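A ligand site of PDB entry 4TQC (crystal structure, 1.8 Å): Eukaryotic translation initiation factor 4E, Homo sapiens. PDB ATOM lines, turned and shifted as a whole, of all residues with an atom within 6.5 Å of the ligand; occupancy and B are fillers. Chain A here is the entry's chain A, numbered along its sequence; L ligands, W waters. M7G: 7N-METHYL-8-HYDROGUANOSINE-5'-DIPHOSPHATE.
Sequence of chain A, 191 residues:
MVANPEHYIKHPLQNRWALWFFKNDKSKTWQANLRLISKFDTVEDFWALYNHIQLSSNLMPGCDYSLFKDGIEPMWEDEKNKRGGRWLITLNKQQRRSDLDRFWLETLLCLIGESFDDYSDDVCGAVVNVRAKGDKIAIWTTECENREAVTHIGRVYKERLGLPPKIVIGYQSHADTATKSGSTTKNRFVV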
ATOM      1  N   PHE A  22     -18.988 -15.361 -10.977  1.00  0.00           N
ATOM      2  CA  PHE A  22     -20.247 -15.198 -11.683  1.00  0.00           C
ATOM      3  C   PHE A  22     -21.138 -16.373 -11.333  1.00  0.00           C
ATOM      4  O   PHE A  22     -20.742 -17.521 -11.492  1.00  0.00           O
ATOM      5  CB  PHE A  22     -20.016 -15.110 -13.192  1.00  0.00           C
ATOM      6  CG  PHE A  22     -21.272 -14.977 -13.996  1.00  0.00           C
ATOM      7  CD1 PHE A  22     -21.667 -13.745 -14.493  1.00  0.00           C
ATOM      8  CD2 PHE A  22     -22.071 -16.080 -14.264  1.00  0.00           C
ATOM      9  CE1 PHE A  22     -22.823 -13.621 -15.236  1.00  0.00           C
ATOM     10  CE2 PHE A  22     -23.230 -15.953 -14.997  1.00  0.00           C
ATOM     11  CZ  PHE A  22     -23.607 -14.731 -15.487  1.00  0.00           C
ATOM     12  N   LYS A  26     -30.547 -16.894 -14.819  1.00  0.00           N
ATOM     13  CA  LYS A  26     -31.212 -16.428 -16.031  1.00  0.00           C
ATOM     14  C   LYS A  26     -32.316 -15.417 -15.733  1.00  0.00           C
ATOM     15  O   LYS A  26     -32.765 -14.698 -16.625  1.00  0.00           O
ATOM     16  CB  LYS A  26     -31.792 -17.619 -16.805  1.00  0.00           C
ATOM     17  CG  LYS A  26     -30.750 -18.629 -17.260  1.00  0.00           C
ATOM     18  CD  LYS A  26     -29.836 -18.060 -18.345  1.00  0.00           C
ATOM     19  CE  LYS A  26     -28.742 -19.030 -18.732  1.00  0.00           C
ATOM     20  NZ  LYS A  26     -27.819 -18.462 -19.750  1.00  0.00           N
ATOM     21  N   TRP A  30     -27.316  -9.995 -17.081  1.00  0.00           N
ATOM     22  CA  TRP A  30     -26.007 -10.644 -16.943  1.00  0.00           C
ATOM     23  C   TRP A  30     -25.084  -9.969 -15.941  1.00  0.00           C
ATOM     24  O   TRP A  30     -24.487 -10.633 -15.089  1.00  0.00           O
ATOM     25  CB  TRP A  30     -25.322 -10.716 -18.306  1.00  0.00           C
ATOM     26  CG  TRP A  30     -24.070 -11.531 -18.308  1.00  0.00           C
ATOM     27  CD1 TRP A  30     -23.972 -12.880 -18.502  1.00  0.00           C
ATOM     28  CD2 TRP A  30     -22.728 -11.061 -18.102  1.00  0.00           C
ATOM     29  NE1 TRP A  30     -22.654 -13.272 -18.434  1.00  0.00           N
ATOM     30  CE2 TRP A  30     -21.876 -12.170 -18.193  1.00  0.00           C
ATOM     31  CE3 TRP A  30     -22.184  -9.800 -17.851  1.00  0.00           C
ATOM     32  CZ2 TRP A  30     -20.494 -12.067 -18.033  1.00  0.00           C
ATOM     33  CZ3 TRP A  30     -20.816  -9.694 -17.695  1.00  0.00           C
ATOM     34  CH2 TRP A  30     -19.988 -10.821 -17.788  1.00  0.00           C
ATOM     35  N   GLN A  31     -24.964  -8.643 -16.026  1.00  0.00           N
ATOM     36  CA  GLN A  31     -24.033  -7.913 -15.167  1.00  0.00           C
ATOM     37  C   GLN A  31     -24.387  -8.030 -13.683  1.00  0.00           C
ATOM     38  O   GLN A  31     -23.530  -7.824 -12.824  1.00  0.00           O
ATOM     39  CB  GLN A  31     -24.002  -6.427 -15.557  1.00  0.00           C
ATOM     40  CG  GLN A  31     -23.168  -6.097 -16.768  1.00  0.00           C
ATOM     41  CD  GLN A  31     -22.942  -4.601 -16.915  1.00  0.00           C
ATOM     42  OE1 GLN A  31     -22.714  -3.891 -15.927  1.00  0.00           O
ATOM     43  NE2 GLN A  31     -23.020  -4.099 -18.141  1.00  0.00           N
ATOM     44  N   GLY A  62     -22.426 -23.726 -14.055  1.00  0.00           N
ATOM     45  CA  GLY A  62     -23.048 -22.504 -14.525  1.00  0.00           C
ATOM     46  C   GLY A  62     -22.236 -21.274 -14.139  1.00  0.00           C
ATOM     47  O   GLY A  62     -22.377 -20.203 -14.737  1.00  0.00           O
ATOM     48  N   ASP A  64     -18.758 -18.884 -13.150  1.00  0.00           N
ATOM     49  CA  ASP A  64     -17.457 -18.538 -13.714  1.00  0.00           C
ATOM     50  C   ASP A  64     -16.514 -18.022 -12.641  1.00  0.00           C
ATOM     51  O   ASP A  64     -16.947 -17.416 -11.651  1.00  0.00           O
ATOM     52  CB  ASP A  64     -17.571 -17.472 -14.808  1.00  0.00           C
ATOM     53  CG  ASP A  64     -18.673 -17.751 -15.809  1.00  0.00           C
ATOM     54  OD1 ASP A  64     -19.079 -18.923 -15.952  1.00  0.00           O
ATOM     55  OD2 ASP A  64     -19.112 -16.790 -16.467  1.00  0.00           O
ATOM     56  N   PRO A  74     -14.518  -8.007 -15.847  1.00  0.00           N
ATOM     57  CA  PRO A  74     -14.513  -9.166 -16.752  1.00  0.00           C
ATOM     58  C   PRO A  74     -15.729  -9.201 -17.670  1.00  0.00           C
ATOM     59  O   PRO A  74     -16.471 -10.185 -17.678  1.00  0.00           O
ATOM     60  CB  PRO A  74     -14.491 -10.349 -15.779  1.00  0.00           C
ATOM     61  CG  PRO A  74     -15.278  -9.864 -14.625  1.00  0.00           C
ATOM     62  CD  PRO A  74     -14.962  -8.386 -14.496  1.00  0.00           C
ATOM     63  N   MET A  75     -15.923  -8.142 -18.440  1.00  0.00           N
ATOM     64  CA  MET A  75     -17.071  -8.031 -19.338  1.00  0.00           C
ATOM     65  C   MET A  75     -16.706  -7.251 -20.598  1.00  0.00           C
ATOM     66  O   MET A  75     -15.802  -6.413 -20.581  1.00  0.00           O
ATOM     67  CB  MET A  75     -18.253  -7.355 -18.623  1.00  0.00           C
ATOM     68  CG  MET A  75     -18.025  -5.895 -18.266  1.00  0.00           C
ATOM     69  SD  MET A  75     -19.347  -5.185 -17.276  1.00  0.00           S
ATOM     70  CE  MET A  75     -19.118  -6.042 -15.728  1.00  0.00           C
ATOM     71  N   TRP A  76     -17.407  -7.551 -21.689  1.00  0.00           N
ATOM     72  CA  TRP A  76     -17.174  -6.879 -22.965  1.00  0.00           C
ATOM     73  C   TRP A  76     -17.246  -5.367 -22.843  1.00  0.00           C
ATOM     74  O   TRP A  76     -16.481  -4.648 -23.474  1.00  0.00           O
ATOM     75  CB  TRP A  76     -18.184  -7.336 -24.009  1.00  0.00           C
ATOM     76  CG  TRP A  76     -18.292  -8.810 -24.179  1.00  0.00           C
ATOM     77  CD1 TRP A  76     -17.283  -9.724 -24.101  1.00  0.00           C
ATOM     78  CD2 TRP A  76     -19.477  -9.553 -24.449  1.00  0.00           C
ATOM     79  NE1 TRP A  76     -17.766 -10.990 -24.313  1.00  0.00           N
ATOM     80  CE2 TRP A  76     -19.124 -10.911 -24.528  1.00  0.00           C
ATOM     81  CE3 TRP A  76     -20.824  -9.195 -24.633  1.00  0.00           C
ATOM     82  CZ2 TRP A  76     -20.054 -11.916 -24.784  1.00  0.00           C
ATOM     83  CZ3 TRP A  76     -21.741 -10.201 -24.884  1.00  0.00           C
ATOM     84  CH2 TRP A  76     -21.350 -11.544 -24.958  1.00  0.00           C
ATOM     85  N   GLU A  77     -18.174  -4.892 -22.013  1.00  0.00           N
ATOM     86  CA  GLU A  77     -18.468  -3.463 -21.917  1.00  0.00           C
ATOM     87  C   GLU A  77     -17.305  -2.628 -21.390  1.00  0.00           C
ATOM     88  O   GLU A  77     -17.285  -1.411 -21.567  1.00  0.00           O
ATOM     89  CB  GLU A  77     -19.688  -3.225 -21.013  1.00  0.00           C
ATOM     90  CG  GLU A  77     -20.980  -3.822 -21.535  1.00  0.00           C
ATOM     91  CD  GLU A  77     -21.208  -5.230 -21.027  1.00  0.00           C
ATOM     92  OE1 GLU A  77     -20.252  -6.026 -21.006  1.00  0.00           O
ATOM     93  OE2 GLU A  77     -22.365  -5.533 -20.661  1.00  0.00           O
ATOM     94  N   ARG A  86     -10.803 -12.922 -27.231  1.00  0.00           N
ATOM     95  CA  ARG A  86     -10.329 -13.974 -26.345  1.00  0.00           C
ATOM     96  C   ARG A  86      -9.837 -15.199 -27.090  1.00  0.00           C
ATOM     97  O   ARG A  86     -10.410 -15.605 -28.095  1.00  0.00           O
ATOM     98  CB  ARG A  86     -11.449 -14.392 -25.390  1.00  0.00           C
ATOM     99  CG  ARG A  86     -12.640 -15.029 -26.088  1.00  0.00           C
ATOM    100  CD  ARG A  86     -13.718 -15.456 -25.130  1.00  0.00           C
ATOM    101  NE  ARG A  86     -14.843 -16.026 -25.861  1.00  0.00           N
ATOM    102  CZ  ARG A  86     -15.821 -16.746 -25.319  1.00  0.00           C
ATOM    103  NH1 ARG A  86     -15.818 -17.007 -24.021  1.00  0.00           N
ATOM    104  NH2 ARG A  86     -16.802 -17.221 -26.082  1.00  0.00           N
ATOM    105  N   ASN A 129     -15.299 -20.937 -17.619  1.00  0.00           N
ATOM    106  CA  ASN A 129     -16.722 -21.249 -17.559  1.00  0.00           C
ATOM    107  C   ASN A 129     -16.905 -22.720 -17.225  1.00  0.00           C
ATOM    108  O   ASN A 129     -16.413 -23.579 -17.955  1.00  0.00           O
ATOM    109  CB  ASN A 129     -17.421 -20.932 -18.878  1.00  0.00           C
ATOM    110  CG  ASN A 129     -17.082 -19.557 -19.422  1.00  0.00           C
ATOM    111  OD1 ASN A 129     -16.421 -19.437 -20.448  1.00  0.00           O
ATOM    112  ND2 ASN A 129     -17.548 -18.521 -18.735  1.00  0.00           N
ATOM    113  N   ARG A 131     -19.407 -25.480 -17.493  1.00  0.00           N
ATOM    114  CA  ARG A 131     -20.613 -25.754 -18.276  1.00  0.00           C
ATOM    115  C   ARG A 131     -20.786 -27.250 -18.511  1.00  0.00           C
ATOM    116  O   ARG A 131     -19.829 -27.942 -18.853  1.00  0.00           O
ATOM    117  CB  ARG A 131     -20.552 -25.020 -19.615  1.00  0.00           C
ATOM    118  CG  ARG A 131     -20.358 -23.521 -19.515  1.00  0.00           C
ATOM    119  CD  ARG A 131     -21.627 -22.812 -19.079  1.00  0.00           C
ATOM    120  NE  ARG A 131     -21.468 -21.356 -19.104  1.00  0.00           N
ATOM    121  CZ  ARG A 131     -20.993 -20.635 -18.086  1.00  0.00           C
ATOM    122  NH1 ARG A 131     -20.634 -21.214 -16.956  1.00  0.00           N
ATOM    123  NH2 ARG A 131     -20.873 -19.320 -18.221  1.00  0.00           N
ATOM    124  N   LYS A 133     -22.194 -28.569 -20.964  1.00  0.00           N
ATOM    125  CA  LYS A 133     -21.926 -28.790 -22.386  1.00  0.00           C
ATOM    126  C   LYS A 133     -20.425 -28.901 -22.670  1.00  0.00           C
ATOM    127  O   LYS A 133     -20.020 -29.335 -23.748  1.00  0.00           O
ATOM    128  CB  LYS A 133     -22.531 -27.676 -23.228  1.00  0.00           C
ATOM    129  CG  LYS A 133     -24.051 -27.575 -23.107  1.00  0.00           C
ATOM    130  CD  LYS A 133     -24.630 -26.603 -24.127  1.00  0.00           C
ATOM    131  CE  LYS A 133     -26.139 -26.501 -23.993  1.00  0.00           C
ATOM    132  NZ  LYS A 133     -26.727 -25.570 -25.004  1.00  0.00           N
ATOM    133  N   GLY A 134     -19.614 -28.501 -21.686  1.00  0.00           N
ATOM    134  CA  GLY A 134     -18.165 -28.552 -21.818  1.00  0.00           C
ATOM    135  C   GLY A 134     -17.551 -27.281 -21.283  1.00  0.00           C
ATOM    136  O   GLY A 134     -17.900 -26.175 -21.700  1.00  0.00           O
ATOM    137  N   LYS A 136     -14.975 -24.219 -20.383  1.00  0.00           N
ATOM    138  CA  LYS A 136     -14.201 -23.330 -21.242  1.00  0.00           C
ATOM    139  C   LYS A 136     -13.223 -22.523 -20.424  1.00  0.00           C
ATOM    140  O   LYS A 136     -13.518 -22.111 -19.299  1.00  0.00           O
ATOM    141  CB  LYS A 136     -15.129 -22.407 -22.031  1.00  0.00           C
ATOM    142  CG  LYS A 136     -16.014 -23.137 -23.039  1.00  0.00           C
ATOM    143  CD  LYS A 136     -16.901 -22.185 -23.825  1.00  0.00           C
ATOM    144  CE  LYS A 136     -18.155 -21.814 -23.055  1.00  0.00           C
ATOM    145  NZ  LYS A 136     -19.098 -21.023 -23.886  1.00  0.00           N
ATOM    146  N   TRP A 140      -8.408 -13.266 -22.218  1.00  0.00           N
ATOM    147  CA  TRP A 140      -8.928 -12.068 -22.858  1.00  0.00           C
ATOM    148  C   TRP A 140      -7.811 -11.051 -23.124  1.00  0.00           C
ATOM    149  O   TRP A 140      -7.019 -10.772 -22.239  1.00  0.00           O
ATOM    150  CB  TRP A 140      -9.992 -11.420 -21.985  1.00  0.00           C
ATOM    151  CG  TRP A 140     -11.293 -12.154 -21.902  1.00  0.00           C
ATOM    152  CD1 TRP A 140     -11.504 -13.488 -22.010  1.00  0.00           C
ATOM    153  CD2 TRP A 140     -12.587 -11.563 -21.686  1.00  0.00           C
ATOM    154  NE1 TRP A 140     -12.842 -13.772 -21.871  1.00  0.00           N
ATOM    155  CE2 TRP A 140     -13.523 -12.604 -21.676  1.00  0.00           C
ATOM    156  CE3 TRP A 140     -13.026 -10.251 -21.499  1.00  0.00           C
ATOM    157  CZ2 TRP A 140     -14.889 -12.380 -21.483  1.00  0.00           C
ATOM    158  CZ3 TRP A 140     -14.381 -10.025 -21.315  1.00  0.00           C
ATOM    159  CH2 TRP A 140     -15.291 -11.085 -21.303  1.00  0.00           C
ATOM    160  N   THR A 177     -18.740 -11.890 -30.749  1.00  0.00           N
ATOM    161  CA  THR A 177     -19.418 -12.750 -29.798  1.00  0.00           C
ATOM    162  C   THR A 177     -20.709 -12.085 -29.313  1.00  0.00           C
ATOM    163  O   THR A 177     -21.715 -12.750 -29.084  1.00  0.00           O
ATOM    164  CB  THR A 177     -18.530 -13.081 -28.586  1.00  0.00           C
ATOM    165  OG1 THR A 177     -17.216 -13.466 -29.025  1.00  0.00           O
ATOM    166  CG2 THR A 177     -19.137 -14.206 -27.754  1.00  0.00           C
HETATM  167  PA  M7G L   1     -21.393 -17.490 -21.926  1.00  0.00           P
HETATM  168  O1A M7G L   1     -19.968 -16.967 -22.035  1.00  0.00           O
HETATM  169  O2A M7G L   1     -21.625 -17.969 -20.512  1.00  0.00           O
HETATM  170  O3A M7G L   1     -21.577 -18.677 -22.982  1.00  0.00           O
HETATM  171  O5' M7G L   1     -22.371 -16.299 -22.257  1.00  0.00           O
HETATM  172  PB  M7G L   1     -22.487 -19.965 -22.820  1.00  0.00           P
HETATM  173  O1B M7G L   1     -23.655 -19.888 -23.789  1.00  0.00           O
HETATM  174  O2B M7G L   1     -21.649 -21.204 -23.146  1.00  0.00           O
HETATM  175  O3B M7G L   1     -23.022 -20.095 -21.413  1.00  0.00           O
HETATM  176  C5' M7G L   1     -23.796 -16.551 -22.397  1.00  0.00           C
HETATM  177  C4' M7G L   1     -24.435 -15.337 -22.386  1.00  0.00           C
HETATM  178  O4' M7G L   1     -23.825 -14.399 -21.285  1.00  0.00           O
HETATM  179  C3' M7G L   1     -24.199 -14.557 -23.713  1.00  0.00           C
HETATM  180  O3' M7G L   1     -25.285 -14.876 -24.709  1.00  0.00           O
HETATM  181  C2' M7G L   1     -24.235 -13.329 -23.394  1.00  0.00           C
HETATM  182  O2' M7G L   1     -25.565 -12.799 -23.621  1.00  0.00           O
HETATM  183  C1' M7G L   1     -23.846 -13.199 -21.748  1.00  0.00           C
HETATM  184  N9  M7G L   1     -22.591 -12.666 -21.615  1.00  0.00           N
HETATM  185  C8  M7G L   1     -21.432 -13.298 -21.587  1.00  0.00           C
HETATM  186  N7  M7G L   1     -20.427 -12.425 -21.445  1.00  0.00           N
HETATM  187  CM7 M7G L   1     -19.019 -12.754 -21.371  1.00  0.00           C
HETATM  188  C5  M7G L   1     -20.957 -11.163 -21.376  1.00  0.00           C
HETATM  189  C6  M7G L   1     -20.376  -9.788 -21.211  1.00  0.00           C
HETATM  190  O6  M7G L   1     -19.183  -9.635 -21.116  1.00  0.00           O
HETATM  191  N1  M7G L   1     -21.231  -8.669 -21.177  1.00  0.00           N
HETATM  192  C2  M7G L   1     -22.643  -8.837 -21.294  1.00  0.00           C
HETATM  193  N2  M7G L   1     -23.496  -7.739 -21.254  1.00  0.00           N
HETATM  194  N3  M7G L   1     -23.207 -10.168 -21.445  1.00  0.00           N
HETATM  195  C4  M7G L   1     -22.327 -11.324 -21.483  1.00  0.00           C
HETATM  196  O   HOH W   1     -17.136 -15.503 -20.926  1.00  0.00           O
HETATM  197  O   HOH W   2     -23.031 -14.306 -27.109  1.00  0.00           O
HETATM  198  O   HOH W   3     -19.438 -15.477 -24.138  1.00  0.00           O
HETATM  199  O   HOH W   4     -25.899  -6.536 -20.039  1.00  0.00           O
HETATM  200  O   HOH W   5     -17.866 -18.586 -22.687  1.00  0.00           O
HETATM  201  O   HOH W   6     -26.187  -9.227 -22.394  1.00  0.00           O
HETATM  202  O   HOH W   7     -17.109 -14.015 -24.011  1.00  0.00           O
HETATM  203  O   HOH W   8     -26.213 -19.167 -24.400  1.00  0.00           O
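The side-chain carboxylate (OE2) of Glu 77 is in hydrogen-bond range of a nitrogen (N2) of the ligand. An oxygen (O2B) of the ligand lies within salt-bridge range of the side-chain amino group (NZ) of Lys 136. NH2 of Arg 131 is in salt-bridge range of O2A of the ligand (2.8 Å). N of Trp 76 lies within hydrogen-bond range of O6 of the ligand (2.8 Å). The indole nitrogen (NE1) of Trp 30 lies close to an oxygen (O4') of the ligand (3.3 Å).
The side-chain carboxylate (OE2) of Glu 77 is in hydrogen-bond range of the side-chain amide nitrogen (NE2) of Gln 31, 3.0 Å away. O of Lys 136 is in hydrogen-bond range of N of Asn 129 (2.7 Å). NH2 of Arg 131 lies close to ND2 of Asn 129, at 3.5 Å. OD1 of Asp 64 is in salt-bridge range of NH2 of Arg 131 (2.9 Å). The guanidinium group of Arg 131 is in hydrogen-bond range of the backbone carbonyl oxygen of Gly 62 (3.0 Å).
Merely in contact with the ligand: Met 75 (3.2 Å). Hydrophobic or aromatic side chains within 4 Å of the ligand: Trp 30, Met 75 and Trp 76. Within 4 Å of the ligand: Trp 30, Met 75, Trp 76, Glu 77, Arg 131 and Lys 136. The nearest printed residue that does not touch the ligand is Trp 140 (4.1 Å).
Water W5 lies within hydrogen-bond range of O1A of the ligand (2.7 Å), OD1 of Asn 129 (2.8 Å), NH1 of Arg 86 (2.9 Å) and NZ of Lys 136 (3.0 Å). Water W2 lies within hydrogen-bond range of O of Thr 177 (2.8 Å) and O3' of the ligand (3.3 Å). Water W7 lies within hydrogen-bond range of NE1 of Trp 76 and NH1 of Arg 86.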
